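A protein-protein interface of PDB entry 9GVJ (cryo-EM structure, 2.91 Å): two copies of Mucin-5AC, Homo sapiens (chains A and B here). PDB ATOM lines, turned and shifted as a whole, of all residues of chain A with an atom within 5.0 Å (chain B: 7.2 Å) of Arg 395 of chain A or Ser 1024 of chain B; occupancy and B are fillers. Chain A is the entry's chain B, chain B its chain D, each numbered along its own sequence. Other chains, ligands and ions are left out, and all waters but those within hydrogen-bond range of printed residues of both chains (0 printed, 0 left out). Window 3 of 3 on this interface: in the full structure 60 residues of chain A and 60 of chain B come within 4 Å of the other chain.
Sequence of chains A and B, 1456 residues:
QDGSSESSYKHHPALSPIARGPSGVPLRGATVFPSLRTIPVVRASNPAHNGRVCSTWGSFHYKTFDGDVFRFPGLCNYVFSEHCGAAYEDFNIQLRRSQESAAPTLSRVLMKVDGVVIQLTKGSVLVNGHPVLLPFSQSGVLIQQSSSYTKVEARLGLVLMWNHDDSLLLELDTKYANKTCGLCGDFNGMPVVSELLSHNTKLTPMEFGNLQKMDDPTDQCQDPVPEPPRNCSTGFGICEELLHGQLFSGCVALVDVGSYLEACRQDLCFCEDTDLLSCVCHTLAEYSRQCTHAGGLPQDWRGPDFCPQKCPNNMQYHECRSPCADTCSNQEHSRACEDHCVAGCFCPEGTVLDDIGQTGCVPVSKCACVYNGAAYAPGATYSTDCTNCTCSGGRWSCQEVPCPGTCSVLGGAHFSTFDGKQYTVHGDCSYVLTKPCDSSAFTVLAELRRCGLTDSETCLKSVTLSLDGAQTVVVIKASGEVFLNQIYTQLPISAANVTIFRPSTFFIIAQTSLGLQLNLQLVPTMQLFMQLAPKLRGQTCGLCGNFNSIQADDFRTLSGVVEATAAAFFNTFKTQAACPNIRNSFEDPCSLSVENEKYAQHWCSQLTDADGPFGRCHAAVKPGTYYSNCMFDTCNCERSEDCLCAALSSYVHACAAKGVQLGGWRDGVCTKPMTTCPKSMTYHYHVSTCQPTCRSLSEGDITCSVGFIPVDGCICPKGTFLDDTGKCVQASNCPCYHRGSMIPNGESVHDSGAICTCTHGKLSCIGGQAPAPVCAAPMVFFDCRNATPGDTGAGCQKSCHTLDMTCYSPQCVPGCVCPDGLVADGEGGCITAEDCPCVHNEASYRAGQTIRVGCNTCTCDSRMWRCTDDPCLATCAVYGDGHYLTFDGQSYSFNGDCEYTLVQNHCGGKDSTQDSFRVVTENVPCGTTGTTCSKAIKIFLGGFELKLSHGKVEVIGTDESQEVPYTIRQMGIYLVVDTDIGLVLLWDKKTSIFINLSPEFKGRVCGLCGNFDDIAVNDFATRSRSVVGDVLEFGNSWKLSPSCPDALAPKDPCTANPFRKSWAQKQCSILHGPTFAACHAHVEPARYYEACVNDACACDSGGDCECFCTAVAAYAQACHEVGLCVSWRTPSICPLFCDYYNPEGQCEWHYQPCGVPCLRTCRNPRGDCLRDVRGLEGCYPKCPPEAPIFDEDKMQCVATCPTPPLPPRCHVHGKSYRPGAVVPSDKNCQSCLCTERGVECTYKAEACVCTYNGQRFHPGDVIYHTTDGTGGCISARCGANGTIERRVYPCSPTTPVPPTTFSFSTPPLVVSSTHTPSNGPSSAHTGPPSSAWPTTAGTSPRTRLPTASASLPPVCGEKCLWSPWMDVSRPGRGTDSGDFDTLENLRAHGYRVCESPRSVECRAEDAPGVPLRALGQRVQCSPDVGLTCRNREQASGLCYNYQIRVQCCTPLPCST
No position is printed for both chains.
N of Trp 396 of chain A lies within hydrogen-bond range of O of Ser 1024 of chain B.
NH1 of Arg 395 of chain A lies close to NH2 of Arg 1025 of chain B (3.1 Å).
The backbone carbonyl oxygen (O) of Trp 396 of chain A sits close to the backbone carbonyl oxygen (O) of Arg 1025 of chain B (3.2 Å).
Among the printed residues, merely in contact across the chains: Ser 329 of chain A with Arg 1023 of chain B, Glu 332 of chain A with Lys 910 of chain B, Arg 395 of chain A with Ser 1024 of chain B and Trp 396 of chain A with Ser 1026 of chain B.
NH2 of Arg 1023 of chain B sits close to O of Trp 1038 of chain B, 3.4 Å away.
The backbone carbonyl oxygen (O) of Cys 907 of chain B is in hydrogen-bond range of the guanidinium group (NH2) of Arg 1025 of chain B.
OG1 of Thr 1022 of chain B is in hydrogen-bond range of O of Ser 1026 of chain B, 3.0 Å away.
The backbone NH of Arg 395 of chain A is in hydrogen-bond range of the side-chain sulfur of Cys 369 of chain A (3.7 Å).
N of Arg 1023 of chain B sits at hydrogen-bond distance from OG of Ser 1037 of chain B, at 2.9 Å.
The side-chain sulfur (SG) of Cys 391 of chain A is disulfide-bonded to the side-chain sulfur (SG) of Cys 369 of chain A.
Of the 13 printed residues of chain B, 5 touch a printed residue of chain A.
Hydrophobic or aromatic side chains of chain A that line the printed part of chain B: Trp 396.
Among the printed residues, 7 pairs touch across the chains.
Printed residues of chain B within 4 Å of Arg 395 of chain A: Ser 1024 and Arg 1025.
Of the printed residues of chain A, Ser 1024 of chain B touches Arg 395 (3.7 Å) and Trp 396 (2.8 Å).
Gly 394 of chain A touches none of the printed residues of chain B.
Of the printed residues of chain A, Arg 1025 of chain B touches Arg 395 and Trp 396.
Printed residues of chain B within 4 Å of Ser 329 of chain A: Arg 1023 (3.4 Å).
The nearest printed residue of chain A that does not touch Ser 1024 of chain B is Gly 394 of chain A (4.1 Å).
The nearest printed residue of chain B that does not touch Glu 332 of chain A is Cys 907 of chain B (5.2 Å).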
ATOM      1  N   SER A 329      -6.336  15.485  -8.908  1.00  0.00           N
ATOM      2  CA  SER A 329      -5.430  14.639  -9.679  1.00  0.00           C
ATOM      3  C   SER A 329      -4.693  13.651  -8.783  1.00  0.00           C
ATOM      4  O   SER A 329      -4.522  12.482  -9.148  1.00  0.00           O
ATOM      5  CB  SER A 329      -4.436  15.505 -10.451  1.00  0.00           C
ATOM      6  OG  SER A 329      -5.106  16.419 -11.303  1.00  0.00           O
ATOM      7  N   GLN A 331      -5.143  12.311  -5.177  1.00  0.00           N
ATOM      8  CA  GLN A 331      -5.952  12.201  -3.972  1.00  0.00           C
ATOM      9  C   GLN A 331      -5.293  11.365  -2.883  1.00  0.00           C
ATOM     10  O   GLN A 331      -5.855  11.243  -1.790  1.00  0.00           O
ATOM     11  CB  GLN A 331      -7.322  11.608  -4.314  1.00  0.00           C
ATOM     12  CG  GLN A 331      -7.869  12.067  -5.653  1.00  0.00           C
ATOM     13  CD  GLN A 331      -9.191  11.416  -5.992  1.00  0.00           C
ATOM     14  OE1 GLN A 331      -9.573  10.413  -5.391  1.00  0.00           O
ATOM     15  NE2 GLN A 331      -9.897  11.983  -6.962  1.00  0.00           N
ATOM     16  N   GLU A 332      -4.122  10.784  -3.153  1.00  0.00           N
ATOM     17  CA  GLU A 332      -3.386  10.005  -2.164  1.00  0.00           C
ATOM     18  C   GLU A 332      -2.023  10.617  -1.862  1.00  0.00           C
ATOM     19  O   GLU A 332      -1.114   9.912  -1.411  1.00  0.00           O
ATOM     20  CB  GLU A 332      -3.227   8.558  -2.635  1.00  0.00           C
ATOM     21  CG  GLU A 332      -4.328   7.629  -2.155  1.00  0.00           C
ATOM     22  CD  GLU A 332      -3.837   6.212  -1.927  1.00  0.00           C
ATOM     23  OE1 GLU A 332      -3.571   5.506  -2.923  1.00  0.00           O
ATOM     24  OE2 GLU A 332      -3.718   5.804  -0.753  1.00  0.00           O
ATOM     25  N   CYS A 369     -12.432  15.420 -14.030  1.00  0.00           N
ATOM     26  CA  CYS A 369     -11.450  14.563 -14.678  1.00  0.00           C
ATOM     27  C   CYS A 369     -10.927  15.247 -15.933  1.00  0.00           C
ATOM     28  O   CYS A 369     -11.637  16.022 -16.578  1.00  0.00           O
ATOM     29  CB  CYS A 369     -12.044  13.194 -15.034  1.00  0.00           C
ATOM     30  SG  CYS A 369     -12.817  12.329 -13.650  1.00  0.00           S
ATOM     31  N   THR A 390     -15.612   6.568 -18.055  1.00  0.00           N
ATOM     32  CA  THR A 390     -16.486   7.512 -17.375  1.00  0.00           C
ATOM     33  C   THR A 390     -15.748   8.138 -16.199  1.00  0.00           C
ATOM     34  O   THR A 390     -14.925   7.493 -15.546  1.00  0.00           O
ATOM     35  CB  THR A 390     -17.774   6.839 -16.878  1.00  0.00           C
ATOM     36  OG1 THR A 390     -18.502   7.751 -16.047  1.00  0.00           O
ATOM     37  CG2 THR A 390     -17.452   5.584 -16.085  1.00  0.00           C
ATOM     38  N   CYS A 391     -16.048   9.407 -15.938  1.00  0.00           N
ATOM     39  CA  CYS A 391     -15.399  10.154 -14.868  1.00  0.00           C
ATOM     40  C   CYS A 391     -16.162   9.944 -13.565  1.00  0.00           C
ATOM     41  O   CYS A 391     -17.357  10.253 -13.483  1.00  0.00           O
ATOM     42  CB  CYS A 391     -15.324  11.640 -15.217  1.00  0.00           C
ATOM     43  SG  CYS A 391     -14.801  12.710 -13.860  1.00  0.00           S
ATOM     44  N   SER A 392     -15.476   9.419 -12.553  1.00  0.00           N
ATOM     45  CA  SER A 392     -16.077   9.168 -11.247  1.00  0.00           C
ATOM     46  C   SER A 392     -15.052   9.471 -10.166  1.00  0.00           C
ATOM     47  O   SER A 392     -13.946   8.921 -10.190  1.00  0.00           O
ATOM     48  CB  SER A 392     -16.566   7.722 -11.132  1.00  0.00           C
ATOM     49  OG  SER A 392     -16.984   7.431  -9.811  1.00  0.00           O
ATOM     50  N   GLY A 393     -15.418  10.344  -9.230  1.00  0.00           N
ATOM     51  CA  GLY A 393     -14.557  10.644  -8.098  1.00  0.00           C
ATOM     52  C   GLY A 393     -13.200  11.193  -8.470  1.00  0.00           C
ATOM     53  O   GLY A 393     -12.231  10.988  -7.732  1.00  0.00           O
ATOM     54  N   GLY A 394     -13.102  11.889  -9.601  1.00  0.00           N
ATOM     55  CA  GLY A 394     -11.833  12.401 -10.070  1.00  0.00           C
ATOM     56  C   GLY A 394     -10.975  11.400 -10.808  1.00  0.00           C
ATOM     57  O   GLY A 394      -9.875  11.758 -11.246  1.00  0.00           O
ATOM     58  N   ARG A 395     -11.434  10.164 -10.963  1.00  0.00           N
ATOM     59  CA  ARG A 395     -10.697   9.135 -11.676  1.00  0.00           C
ATOM     60  C   ARG A 395     -11.511   8.656 -12.870  1.00  0.00           C
ATOM     61  O   ARG A 395     -12.655   9.064 -13.079  1.00  0.00           O
ATOM     62  CB  ARG A 395     -10.350   7.963 -10.750  1.00  0.00           C
ATOM     63  CG  ARG A 395      -9.114   8.209  -9.903  1.00  0.00           C
ATOM     64  CD  ARG A 395      -9.199   7.498  -8.566  1.00  0.00           C
ATOM     65  NE  ARG A 395      -8.024   7.761  -7.742  1.00  0.00           N
ATOM     66  CZ  ARG A 395      -7.880   7.353  -6.489  1.00  0.00           C
ATOM     67  NH1 ARG A 395      -8.823   6.655  -5.877  1.00  0.00           N
ATOM     68  NH2 ARG A 395      -6.762   7.651  -5.835  1.00  0.00           N
ATOM     69  N   TRP A 396     -10.899   7.783 -13.664  1.00  0.00           N
ATOM     70  CA  TRP A 396     -11.511   7.250 -14.873  1.00  0.00           C
ATOM     71  C   TRP A 396     -11.802   5.769 -14.672  1.00  0.00           C
ATOM     72  O   TRP A 396     -10.902   4.999 -14.318  1.00  0.00           O
ATOM     73  CB  TRP A 396     -10.600   7.458 -16.082  1.00  0.00           C
ATOM     74  CG  TRP A 396     -10.593   8.864 -16.601  1.00  0.00           C
ATOM     75  CD1 TRP A 396      -9.562   9.754 -16.538  1.00  0.00           C
ATOM     76  CD2 TRP A 396     -11.667   9.540 -17.264  1.00  0.00           C
ATOM     77  NE1 TRP A 396      -9.927  10.943 -17.121  1.00  0.00           N
ATOM     78  CE2 TRP A 396     -11.215  10.837 -17.574  1.00  0.00           C
ATOM     79  CE3 TRP A 396     -12.965   9.175 -17.627  1.00  0.00           C
ATOM     80  CZ2 TRP A 396     -12.015  11.770 -18.228  1.00  0.00           C
ATOM     81  CZ3 TRP A 396     -13.759  10.101 -18.274  1.00  0.00           C
ATOM     82  CH2 TRP A 396     -13.282  11.384 -18.568  1.00  0.00           C
ATOM     83  N   SER A 397     -13.052   5.376 -14.899  1.00  0.00           N
ATOM     84  CA  SER A 397     -13.454   3.974 -14.900  1.00  0.00           C
ATOM     85  C   SER A 397     -13.670   3.569 -16.353  1.00  0.00           C
ATOM     86  O   SER A 397     -14.581   4.076 -17.012  1.00  0.00           O
ATOM     87  CB  SER A 397     -14.715   3.763 -14.067  1.00  0.00           C
ATOM     88  OG  SER A 397     -14.660   4.502 -12.861  1.00  0.00           O
ATOM     89  N   CYS B 907      -2.499   0.655  -6.297  1.00  0.00           N
ATOM     90  CA  CYS B 907      -2.977   1.701  -7.198  1.00  0.00           C
ATOM     91  C   CYS B 907      -4.501   1.709  -7.279  1.00  0.00           C
ATOM     92  O   CYS B 907      -5.141   2.722  -6.981  1.00  0.00           O
ATOM     93  CB  CYS B 907      -2.360   1.512  -8.588  1.00  0.00           C
ATOM     94  SG  CYS B 907      -0.580   1.206  -8.565  1.00  0.00           S
ATOM     95  N   GLY B 908      -5.092   0.587  -7.681  1.00  0.00           N
ATOM     96  CA  GLY B 908      -6.535   0.466  -7.730  1.00  0.00           C
ATOM     97  C   GLY B 908      -7.094  -0.194  -6.488  1.00  0.00           C
ATOM     98  O   GLY B 908      -6.858  -1.382  -6.249  1.00  0.00           O
ATOM     99  N   GLY B 909      -7.840   0.567  -5.689  1.00  0.00           N
ATOM    100  CA  GLY B 909      -8.341   0.106  -4.414  1.00  0.00           C
ATOM    101  C   GLY B 909      -7.403   0.363  -3.253  1.00  0.00           C
ATOM    102  O   GLY B 909      -7.867   0.588  -2.129  1.00  0.00           O
ATOM    103  N   LYS B 910      -6.093   0.325  -3.498  1.00  0.00           N
ATOM    104  CA  LYS B 910      -5.061   0.656  -2.516  1.00  0.00           C
ATOM    105  C   LYS B 910      -5.089  -0.260  -1.296  1.00  0.00           C
ATOM    106  O   LYS B 910      -4.606   0.120  -0.224  1.00  0.00           O
ATOM    107  CB  LYS B 910      -5.162   2.121  -2.077  1.00  0.00           C
ATOM    108  N   ALA B1021      -1.105   4.381 -18.982  1.00  0.00           N
ATOM    109  CA  ALA B1021      -2.183   4.766 -18.083  1.00  0.00           C
ATOM    110  C   ALA B1021      -1.719   5.880 -17.156  1.00  0.00           C
ATOM    111  O   ALA B1021      -0.658   5.786 -16.534  1.00  0.00           O
ATOM    112  CB  ALA B1021      -2.651   3.561 -17.270  1.00  0.00           C
ATOM    113  N   THR B1022      -2.520   6.938 -17.065  1.00  0.00           N
ATOM    114  CA  THR B1022      -2.178   8.084 -16.240  1.00  0.00           C
ATOM    115  C   THR B1022      -2.490   7.793 -14.774  1.00  0.00           C
ATOM    116  O   THR B1022      -2.940   6.704 -14.406  1.00  0.00           O
ATOM    117  CB  THR B1022      -2.926   9.324 -16.721  1.00  0.00           C
ATOM    118  OG1 THR B1022      -4.329   9.039 -16.797  1.00  0.00           O
ATOM    119  CG2 THR B1022      -2.431   9.745 -18.093  1.00  0.00           C
ATOM    120  N   ARG B1023      -2.236   8.786 -13.919  1.00  0.00           N
ATOM    121  CA  ARG B1023      -2.599   8.659 -12.512  1.00  0.00           C
ATOM    122  C   ARG B1023      -4.108   8.575 -12.340  1.00  0.00           C
ATOM    123  O   ARG B1023      -4.594   7.927 -11.406  1.00  0.00           O
ATOM    124  CB  ARG B1023      -2.022   9.835 -11.720  1.00  0.00           C
ATOM    125  CG  ARG B1023      -2.529   9.958 -10.295  1.00  0.00           C
ATOM    126  CD  ARG B1023      -1.405   9.749  -9.295  1.00  0.00           C
ATOM    127  NE  ARG B1023      -0.379  10.779  -9.402  1.00  0.00           N
ATOM    128  CZ  ARG B1023       0.836  10.683  -8.878  1.00  0.00           C
ATOM    129  NH1 ARG B1023       1.214   9.612  -8.201  1.00  0.00           N
ATOM    130  NH2 ARG B1023       1.692  11.687  -9.039  1.00  0.00           N
ATOM    131  N   SER B1024      -4.864   9.200 -13.241  1.00  0.00           N
ATOM    132  CA  SER B1024      -6.320   9.143 -13.231  1.00  0.00           C
ATOM    133  C   SER B1024      -6.865   7.832 -13.784  1.00  0.00           C
ATOM    134  O   SER B1024      -8.073   7.740 -14.024  1.00  0.00           O
ATOM    135  CB  SER B1024      -6.896  10.317 -14.025  1.00  0.00           C
ATOM    136  OG  SER B1024      -6.426  11.552 -13.516  1.00  0.00           O
ATOM    137  N   ARG B1025      -6.003   6.836 -14.002  1.00  0.00           N
ATOM    138  CA  ARG B1025      -6.413   5.507 -14.456  1.00  0.00           C
ATOM    139  C   ARG B1025      -7.080   5.566 -15.831  1.00  0.00           C
ATOM    140  O   ARG B1025      -8.167   5.027 -16.045  1.00  0.00           O
ATOM    141  CB  ARG B1025      -7.326   4.831 -13.429  1.00  0.00           C
ATOM    142  CG  ARG B1025      -6.710   4.707 -12.048  1.00  0.00           C
ATOM    143  CD  ARG B1025      -7.711   4.170 -11.042  1.00  0.00           C
ATOM    144  NE  ARG B1025      -7.221   4.292  -9.674  1.00  0.00           N
ATOM    145  CZ  ARG B1025      -7.976   4.155  -8.592  1.00  0.00           C
ATOM    146  NH1 ARG B1025      -9.269   3.889  -8.682  1.00  0.00           N
ATOM    147  NH2 ARG B1025      -7.419   4.284  -7.392  1.00  0.00           N
ATOM    148  N   SER B1026      -6.411   6.229 -16.770  1.00  0.00           N
ATOM    149  CA  SER B1026      -6.876   6.303 -18.149  1.00  0.00           C
ATOM    150  C   SER B1026      -5.680   6.209 -19.080  1.00  0.00           C
ATOM    151  O   SER B1026      -4.683   6.911 -18.885  1.00  0.00           O
ATOM    152  CB  SER B1026      -7.650   7.598 -18.408  1.00  0.00           C
ATOM    153  OG  SER B1026      -6.768   8.697 -18.562  1.00  0.00           O
ATOM    154  N   VAL B1027      -5.781   5.349 -20.089  1.00  0.00           N
ATOM    155  CA  VAL B1027      -4.704   5.174 -21.058  1.00  0.00           C
ATOM    156  C   VAL B1027      -4.802   6.284 -22.099  1.00  0.00           C
ATOM    157  O   VAL B1027      -5.846   6.461 -22.735  1.00  0.00           O
ATOM    158  CB  VAL B1027      -4.772   3.789 -21.717  1.00  0.00           C
ATOM    159  CG1 VAL B1027      -3.865   3.735 -22.935  1.00  0.00           C
ATOM    160  CG2 VAL B1027      -4.398   2.708 -20.716  1.00  0.00           C
ATOM    161  N   SER B1037       1.317  13.337 -15.571  1.00  0.00           N
ATOM    162  CA  SER B1037       0.326  12.906 -14.593  1.00  0.00           C
ATOM    163  C   SER B1037       0.943  12.195 -13.395  1.00  0.00           C
ATOM    164  O   SER B1037       0.245  11.993 -12.396  1.00  0.00           O
ATOM    165  CB  SER B1037      -0.701  11.990 -15.260  1.00  0.00           C
ATOM    166  OG  SER B1037      -0.359  10.628 -15.077  1.00  0.00           O
ATOM    167  N   TRP B1038       2.219  11.820 -13.462  1.00  0.00           N
ATOM    168  CA  TRP B1038       2.857  11.038 -12.410  1.00  0.00           C
ATOM    169  C   TRP B1038       3.833  11.850 -11.566  1.00  0.00           C
ATOM    170  O   TRP B1038       4.585  11.265 -10.780  1.00  0.00           O
ATOM    171  CB  TRP B1038       3.569   9.827 -13.014  1.00  0.00           C
ATOM    172  CG  TRP B1038       2.631   8.729 -13.391  1.00  0.00           C
ATOM    173  CD1 TRP B1038       2.303   8.330 -14.652  1.00  0.00           C
ATOM    174  CD2 TRP B1038       1.887   7.892 -12.500  1.00  0.00           C
ATOM    175  NE1 TRP B1038       1.404   7.294 -14.603  1.00  0.00           N
ATOM    176  CE2 TRP B1038       1.132   7.006 -13.291  1.00  0.00           C
ATOM    177  CE3 TRP B1038       1.787   7.804 -11.108  1.00  0.00           C
ATOM    178  CZ2 TRP B1038       0.290   6.046 -12.739  1.00  0.00           C
ATOM    179  CZ3 TRP B1038       0.951   6.851 -10.562  1.00  0.00           C
ATOM    180  CH2 TRP B1038       0.213   5.984 -11.375  1.00  0.00           C
